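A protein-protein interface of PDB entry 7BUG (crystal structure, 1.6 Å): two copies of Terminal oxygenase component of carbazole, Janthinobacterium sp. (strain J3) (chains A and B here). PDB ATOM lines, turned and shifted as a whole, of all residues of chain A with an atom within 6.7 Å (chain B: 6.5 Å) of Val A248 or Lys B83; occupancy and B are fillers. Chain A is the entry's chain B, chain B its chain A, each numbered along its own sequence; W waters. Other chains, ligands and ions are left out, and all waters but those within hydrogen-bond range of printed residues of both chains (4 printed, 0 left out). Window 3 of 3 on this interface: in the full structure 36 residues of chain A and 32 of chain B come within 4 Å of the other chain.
Of the 11 printed residues of chain A, 6 touch a printed residue of chain B. Of the 11 printed residues of chain B, 7 touch a printed residue of chain A. Along chain B the printed residues that touch a printed residue of chain A span positions 81 to 108. Among the printed residues, 15 pairs touch across the chains.
The side-chain amino group (NZ) of Lys A188 lies within salt-bridge range of the side-chain carboxylate (OE2) of Glu B81, at 2.9 Å. The side-chain carboxylate (OE1) of Glu B81 sits at hydrogen-bond distance from the side-chain hydroxyl (OH) of Tyr A185 (2.5 Å).
The side-chain hydroxyl (OG1) of Thr B84 lies within hydrogen-bond range of the side-chain hydroxyl (OG1) of Thr B87, at 2.7 Å. NZ of Lys B83 is in salt-bridge range of OE1 of Glu B81. The side-chain sulfur (SG) of Cys B82 lies close to the backbone carbonyl oxygen (O) of Thr B87, at 3.8 Å. The backbone carbonyl oxygen (O) of Tyr A185 sits close to the side-chain amino group (NZ) of Lys A188. OG1 of Thr B89 is in hydrogen-bond range of OG1 of Thr B96 (2.9 Å). The backbone NH of Gly A241 sits at hydrogen-bond distance from the backbone carbonyl oxygen of Arg A249 (2.8 Å).
Water W1 bridges NZ of Lys A188 (2.7 Å) and NZ of Lys B79 (3.4 Å). Water W2 bridges NZ of Lys B83 (2.8 Å) and NH1 of Arg A249 (3.0 Å). Water W3 lies within hydrogen-bond range of the backbone carbonyl oxygen of Leu B108 and the backbone NH of Thr A242. Water W4 lies within hydrogen-bond range of OE2 of Glu B81 (2.9 Å) and NZ of Lys A188 (2.9 Å).
Tyr A185 touches Lys B83. Tyr A185 touches Thr B89 (OH to CG2, 3.8 Å). CD1 of Leu B108 touches OH of Tyr A185, 3.7 Å away. O of Thr A242 touches CD2 of Leu B108, 3.1 Å away. Thr B87 touches Ile A243 (OG1 to CD1, 3.9 Å). Ile A243 touches Thr B89 (CD1 to OG1, 3.6 Å). Ile A243 touches Thr B96 (CD1 to CG2, 3.8 Å). O of Lys B83 touches CG1 of Val A248 (3.9 Å). Val A248 touches Thr B84. Arg A249 touches Lys B83 (CB to CE, 3.9 Å).
Of the printed residues of chain B, Thr A242 touches Leu B108 (3.1 Å). Of chain B, only Lys B83 and Thr B84 come within 4 Å of Val A248. Of chain A, only Tyr A185 (3.5 Å), Ile A243 (3.8 Å), Val A248 (3.9 Å) and Arg A249 (3.9 Å) come within 4 Å of Lys B83. Of the printed residues of chain A, Thr B89 touches Tyr A185 (3.8 Å) and Ile A243 (3.6 Å). The nearest residue of chain B that does not touch Val A248 is Leu B108 (4.1 Å). The nearest residue of chain A that does not touch Lys B83 is Lys A188 (4.6 Å). The nearest printed residue of chain B that does not touch Arg A249 is Leu B108 (4.5 Å).
No position is printed for both chains. Of the 15 pairs that touch across the chains among the printed residues, none has its exchanged pair printed and touching as well.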
ATOM      1  N   TYR A 185      10.699  28.175  23.811  1.00  0.00           N
ATOM      2  CA  TYR A 185       9.540  28.251  22.883  1.00  0.00           C
ATOM      3  C   TYR A 185       9.016  29.688  22.780  1.00  0.00           C
ATOM      4  O   TYR A 185       8.609  30.108  21.685  1.00  0.00           O
ATOM      5  CB  TYR A 185       8.489  27.268  23.325  1.00  0.00           C
ATOM      6  CG  TYR A 185       7.341  27.167  22.381  1.00  0.00           C
ATOM      7  CD1 TYR A 185       7.463  26.454  21.207  1.00  0.00           C
ATOM      8  CD2 TYR A 185       6.156  27.829  22.628  1.00  0.00           C
ATOM      9  CE1 TYR A 185       6.425  26.405  20.274  1.00  0.00           C
ATOM     10  CE2 TYR A 185       5.110  27.773  21.724  1.00  0.00           C
ATOM     11  CZ  TYR A 185       5.251  27.058  20.549  1.00  0.00           C
ATOM     12  OH  TYR A 185       4.224  27.035  19.623  1.00  0.00           O
ATOM     13  N   LYS A 188      10.775  32.152  20.097  1.00  0.00           N
ATOM     14  CA  LYS A 188      10.921  31.614  18.701  1.00  0.00           C
ATOM     15  C   LYS A 188      10.762  32.749  17.678  1.00  0.00           C
ATOM     16  O   LYS A 188      11.316  32.598  16.581  1.00  0.00           O
ATOM     17  CB  LYS A 188       9.924  30.502  18.442  1.00  0.00           C
ATOM     18  CG  LYS A 188       8.438  30.816  18.557  1.00  0.00           C
ATOM     19  CD  LYS A 188       7.550  29.598  18.559  1.00  0.00           C
ATOM     20  CE  LYS A 188       6.072  29.926  18.698  1.00  0.00           C
ATOM     21  NZ  LYS A 188       5.842  30.567  20.026  1.00  0.00           N
ATOM     22  N   GLU A 240      11.523  20.822  14.380  1.00  0.00           N
ATOM     23  CA  GLU A 240      10.230  20.642  13.667  1.00  0.00           C
ATOM     24  C   GLU A 240       9.209  20.197  14.700  1.00  0.00           C
ATOM     25  O   GLU A 240       9.195  19.022  15.063  1.00  0.00           O
ATOM     26  CB  GLU A 240      10.433  19.677  12.495  1.00  0.00           C
ATOM     27  CG  GLU A 240      11.285  20.300  11.403  1.00  0.00           C
ATOM     28  CD  GLU A 240      11.561  19.345  10.256  1.00  0.00           C
ATOM     29  OE1 GLU A 240      10.868  19.456   9.236  1.00  0.00           O
ATOM     30  OE2 GLU A 240      12.449  18.478  10.413  1.00  0.00           O
ATOM     31  N   GLY A 241       8.372  21.127  15.173  1.00  0.00           N
ATOM     32  CA  GLY A 241       7.342  20.786  16.165  1.00  0.00           C
ATOM     33  C   GLY A 241       6.113  20.238  15.484  1.00  0.00           C
ATOM     34  O   GLY A 241       5.688  20.842  14.494  1.00  0.00           O
ATOM     35  N   THR A 242       5.562  19.159  16.010  1.00  0.00           N
ATOM     36  CA  THR A 242       4.485  18.410  15.364  1.00  0.00           C
ATOM     37  C   THR A 242       3.229  18.359  16.229  1.00  0.00           C
ATOM     38  O   THR A 242       3.276  18.222  17.479  1.00  0.00           O
ATOM     39  CB  THR A 242       4.892  16.998  14.960  1.00  0.00           C
ATOM     40  OG1 THR A 242       5.223  16.256  16.129  1.00  0.00           O
ATOM     41  CG2 THR A 242       6.066  16.953  14.005  1.00  0.00           C
ATOM     42  N   ILE A 243       2.104  18.346  15.551  1.00  0.00           N
ATOM     43  CA  ILE A 243       0.782  18.061  16.162  1.00  0.00           C
ATOM     44  C   ILE A 243       0.155  16.965  15.298  1.00  0.00           C
ATOM     45  O   ILE A 243      -0.001  17.235  14.094  1.00  0.00           O
ATOM     46  CB  ILE A 243      -0.114  19.299  16.281  1.00  0.00           C
ATOM     47  CG1 ILE A 243       0.516  20.349  17.213  1.00  0.00           C
ATOM     48  CG2 ILE A 243      -1.500  18.881  16.740  1.00  0.00           C
ATOM     49  CD1 ILE A 243      -0.190  21.690  17.207  1.00  0.00           C
ATOM     50  N   GLU A 246       2.066  16.122  12.149  1.00  0.00           N
ATOM     51  CA  GLU A 246       2.190  17.149  11.080  1.00  0.00           C
ATOM     52  C   GLU A 246       3.052  18.287  11.604  1.00  0.00           C
ATOM     53  O   GLU A 246       2.800  18.755  12.772  1.00  0.00           O
ATOM     54  CB  GLU A 246       0.822  17.661  10.632  1.00  0.00           C
ATOM     55  CG  GLU A 246      -0.119  16.539  10.165  1.00  0.00           C
ATOM     56  CD  GLU A 246       0.394  15.622   9.057  1.00  0.00           C
ATOM     57  OE1 GLU A 246       0.223  14.366   9.164  1.00  0.00           O
ATOM     58  OE2 GLU A 246       0.992  16.151   8.097  1.00  0.00           O
ATOM     59  N   VAL A 247       4.023  18.737  10.810  1.00  0.00           N
ATOM     60  CA  VAL A 247       4.885  19.871  11.237  1.00  0.00           C
ATOM     61  C   VAL A 247       4.034  21.139  11.253  1.00  0.00           C
ATOM     62  O   VAL A 247       3.482  21.504  10.214  1.00  0.00           O
ATOM     63  CB  VAL A 247       6.146  20.035  10.363  1.00  0.00           C
ATOM     64  CG1 VAL A 247       6.974  21.251  10.798  1.00  0.00           C
ATOM     65  CG2 VAL A 247       6.939  18.737  10.411  1.00  0.00           C
ATOM     66  N   VAL A 248       3.947  21.829  12.397  1.00  0.00           N
ATOM     67  CA  VAL A 248       3.167  23.091  12.514  1.00  0.00           C
ATOM     68  C   VAL A 248       4.078  24.267  12.863  1.00  0.00           C
ATOM     69  O   VAL A 248       3.623  25.399  12.782  1.00  0.00           O
ATOM     70  CB  VAL A 248       2.055  22.953  13.566  1.00  0.00           C
ATOM     71  CG1 VAL A 248       1.060  21.858  13.191  1.00  0.00           C
ATOM     72  CG2 VAL A 248       2.680  22.645  14.943  1.00  0.00           C
ATOM     73  N   ARG A 249       5.325  24.039  13.227  1.00  0.00           N
ATOM     74  CA  ARG A 249       6.214  25.137  13.615  1.00  0.00           C
ATOM     75  C   ARG A 249       7.664  24.689  13.511  1.00  0.00           C
ATOM     76  O   ARG A 249       7.953  23.608  13.940  1.00  0.00           O
ATOM     77  CB  ARG A 249       5.906  25.587  15.048  1.00  0.00           C
ATOM     78  CG  ARG A 249       6.865  26.667  15.537  1.00  0.00           C
ATOM     79  CD  ARG A 249       6.666  28.020  14.910  1.00  0.00           C
ATOM     80  NE  ARG A 249       7.873  28.826  14.917  1.00  0.00           N
ATOM     81  CZ  ARG A 249       7.895  30.156  14.959  1.00  0.00           C
ATOM     82  NH1 ARG A 249       6.776  30.861  15.113  1.00  0.00           N
ATOM     83  NH2 ARG A 249       9.047  30.793  14.943  1.00  0.00           N
ATOM     84  N   GLU A 250       8.516  25.526  12.956  1.00  0.00           N
ATOM     85  CA  GLU A 250       9.968  25.225  12.937  1.00  0.00           C
ATOM     86  C   GLU A 250      10.710  26.100  13.924  1.00  0.00           C
ATOM     87  O   GLU A 250      10.269  27.236  14.189  1.00  0.00           O
ATOM     88  CB  GLU A 250      10.586  25.461  11.564  1.00  0.00           C
ATOM     89  CG  GLU A 250      10.109  24.478  10.549  1.00  0.00           C
ATOM     90  CD  GLU A 250      10.899  24.754   9.282  1.00  0.00           C
ATOM     91  OE1 GLU A 250      11.831  23.988   9.019  1.00  0.00           O
ATOM     92  OE2 GLU A 250      10.665  25.824   8.671  1.00  0.00           O
ATOM     93  N   LYS B  79      -1.676  34.513  25.044  1.00  0.00           N
ATOM     94  CA  LYS B  79      -1.183  34.474  23.658  1.00  0.00           C
ATOM     95  C   LYS B  79      -1.713  33.206  23.001  1.00  0.00           C
ATOM     96  O   LYS B  79      -1.172  32.130  23.194  1.00  0.00           O
ATOM     97  CB  LYS B  79       0.340  34.500  23.583  1.00  0.00           C
ATOM     98  CG  LYS B  79       0.880  34.508  22.151  1.00  0.00           C
ATOM     99  CD  LYS B  79       2.394  34.549  22.081  1.00  0.00           C
ATOM    100  CE  LYS B  79       2.956  34.629  20.667  1.00  0.00           C
ATOM    101  NZ  LYS B  79       2.763  33.383  19.871  1.00  0.00           N
ATOM    102  N   GLU B  81      -2.383  30.368  20.567  1.00  0.00           N
ATOM    103  CA  GLU B  81      -1.704  29.667  19.448  1.00  0.00           C
ATOM    104  C   GLU B  81      -2.572  28.497  19.050  1.00  0.00           C
ATOM    105  O   GLU B  81      -2.503  27.438  19.679  1.00  0.00           O
ATOM    106  CB  GLU B  81      -0.312  29.205  19.863  1.00  0.00           C
ATOM    107  CG  GLU B  81       0.693  30.318  20.041  1.00  0.00           C
ATOM    108  CD  GLU B  81       2.157  29.882  20.130  1.00  0.00           C
ATOM    109  OE1 GLU B  81       2.472  28.794  19.603  1.00  0.00           O
ATOM    110  OE2 GLU B  81       2.969  30.689  20.617  1.00  0.00           O
ATOM    111  N   CYS B  82      -3.430  28.646  18.046  1.00  0.00           N
ATOM    112  CA  CYS B  82      -4.196  27.477  17.542  1.00  0.00           C
ATOM    113  C   CYS B  82      -3.509  27.040  16.270  1.00  0.00           C
ATOM    114  O   CYS B  82      -3.628  27.785  15.236  1.00  0.00           O
ATOM    115  CB  CYS B  82      -5.659  27.809  17.297  1.00  0.00           C
ATOM    116  SG  CYS B  82      -6.604  28.102  18.823  1.00  0.00           S
ATOM    117  N   LYS B  83      -2.730  25.969  16.355  1.00  0.00           N
ATOM    118  CA  LYS B  83      -1.809  25.636  15.244  1.00  0.00           C
ATOM    119  C   LYS B  83      -2.443  24.593  14.343  1.00  0.00           C
ATOM    120  O   LYS B  83      -1.923  24.429  13.214  1.00  0.00           O
ATOM    121  CB  LYS B  83      -0.473  25.180  15.801  1.00  0.00           C
ATOM    122  CG  LYS B  83       0.112  26.207  16.747  1.00  0.00           C
ATOM    123  CD  LYS B  83       1.539  25.915  17.208  1.00  0.00           C
ATOM    124  CE  LYS B  83       2.556  26.839  16.596  1.00  0.00           C
ATOM    125  NZ  LYS B  83       2.242  28.256  16.802  1.00  0.00           N
ATOM    126  N   THR B  84      -3.437  23.861  14.833  1.00  0.00           N
ATOM    127  CA  THR B  84      -4.352  23.058  13.988  1.00  0.00           C
ATOM    128  C   THR B  84      -5.792  23.419  14.359  1.00  0.00           C
ATOM    129  O   THR B  84      -6.037  23.916  15.482  1.00  0.00           O
ATOM    130  CB  THR B  84      -4.112  21.558  14.105  1.00  0.00           C
ATOM    131  OG1 THR B  84      -4.623  21.033  15.334  1.00  0.00           O
ATOM    132  CG2 THR B  84      -2.648  21.221  13.933  1.00  0.00           C
ATOM    133  N   LYS B  85      -6.732  23.123  13.471  1.00  0.00           N
ATOM    134  CA  LYS B  85      -8.175  23.391  13.680  1.00  0.00           C
ATOM    135  C   LYS B  85      -8.615  22.800  15.017  1.00  0.00           C
ATOM    136  O   LYS B  85      -9.405  23.427  15.732  1.00  0.00           O
ATOM    137  CB  LYS B  85      -8.969  22.676  12.568  1.00  0.00           C
ATOM    138  CG  LYS B  85     -10.180  23.410  12.052  1.00  0.00           C
ATOM    139  CD  LYS B  85     -10.842  22.775  10.821  1.00  0.00           C
ATOM    140  CE  LYS B  85     -11.218  21.312  11.009  1.00  0.00           C
ATOM    141  NZ  LYS B  85     -11.985  20.730   9.857  1.00  0.00           N
ATOM    142  N   THR B  87      -6.943  21.905  17.780  1.00  0.00           N
ATOM    143  CA  THR B  87      -6.112  22.006  19.000  1.00  0.00           C
ATOM    144  C   THR B  87      -5.830  23.455  19.396  1.00  0.00           C
ATOM    145  O   THR B  87      -5.981  24.397  18.608  1.00  0.00           O
ATOM    146  CB  THR B  87      -4.777  21.251  18.904  1.00  0.00           C
ATOM    147  OG1 THR B  87      -3.993  21.843  17.875  1.00  0.00           O
ATOM    148  CG2 THR B  87      -4.972  19.766  18.651  1.00  0.00           C
ATOM    149  N   ILE B  88      -5.337  23.612  20.610  1.00  0.00           N
ATOM    150  CA  ILE B  88      -4.693  24.882  21.037  1.00  0.00           C
ATOM    151  C   ILE B  88      -3.373  24.508  21.698  1.00  0.00           C
ATOM    152  O   ILE B  88      -3.345  23.480  22.427  1.00  0.00           O
ATOM    153  CB  ILE B  88      -5.604  25.746  21.959  1.00  0.00           C
ATOM    154  CG1 ILE B  88      -4.932  27.072  22.348  1.00  0.00           C
ATOM    155  CG2 ILE B  88      -6.091  24.951  23.142  1.00  0.00           C
ATOM    156  CD1 ILE B  88      -5.882  28.109  22.970  1.00  0.00           C
ATOM    157  N   THR B  89      -2.338  25.319  21.480  1.00  0.00           N
ATOM    158  CA  THR B  89      -0.984  25.089  21.999  1.00  0.00           C
ATOM    159  C   THR B  89      -0.721  26.195  23.027  1.00  0.00           C
ATOM    160  O   THR B  89      -0.780  27.394  22.637  1.00  0.00           O
ATOM    161  CB  THR B  89       0.033  25.122  20.838  1.00  0.00           C
ATOM    162  OG1 THR B  89      -0.276  24.006  20.000  1.00  0.00           O
ATOM    163  CG2 THR B  89       1.461  25.087  21.309  1.00  0.00           C
ATOM    164  N   THR B  96      -0.080  20.978  24.113  1.00  0.00           N
ATOM    165  CA  THR B  96      -1.134  21.103  23.105  1.00  0.00           C
ATOM    166  C   THR B  96      -2.329  20.226  23.483  1.00  0.00           C
ATOM    167  O   THR B  96      -2.148  19.002  23.730  1.00  0.00           O
ATOM    168  CB  THR B  96      -0.564  20.707  21.745  1.00  0.00           C
ATOM    169  OG1 THR B  96       0.492  21.633  21.460  1.00  0.00           O
ATOM    170  CG2 THR B  96      -1.615  20.765  20.658  1.00  0.00           C
ATOM    171  N   LEU B 108       5.110  20.434  21.977  1.00  0.00           N
ATOM    172  CA  LEU B 108       6.079  20.768  20.904  1.00  0.00           C
ATOM    173  C   LEU B 108       7.501  20.797  21.446  1.00  0.00           C
ATOM    174  O   LEU B 108       8.428  20.442  20.711  1.00  0.00           O
ATOM    175  CB  LEU B 108       5.745  22.072  20.177  1.00  0.00           C
ATOM    176  CG  LEU B 108       4.332  22.202  19.599  1.00  0.00           C
ATOM    177  CD1 LEU B 108       4.252  23.406  18.679  1.00  0.00           C
ATOM    178  CD2 LEU B 108       3.833  20.965  18.900  1.00  0.00           C
HETATM  179  O   HOH W   1       6.139  33.256  19.645  1.00  0.00           O
HETATM  180  O   HOH W   2       3.899  30.038  15.515  1.00  0.00           O
HETATM  181  O   HOH W   3       7.699  18.565  18.647  1.00  0.00           O
HETATM  182  O   HOH W   4       4.867  31.744  22.532  1.00  0.00           O
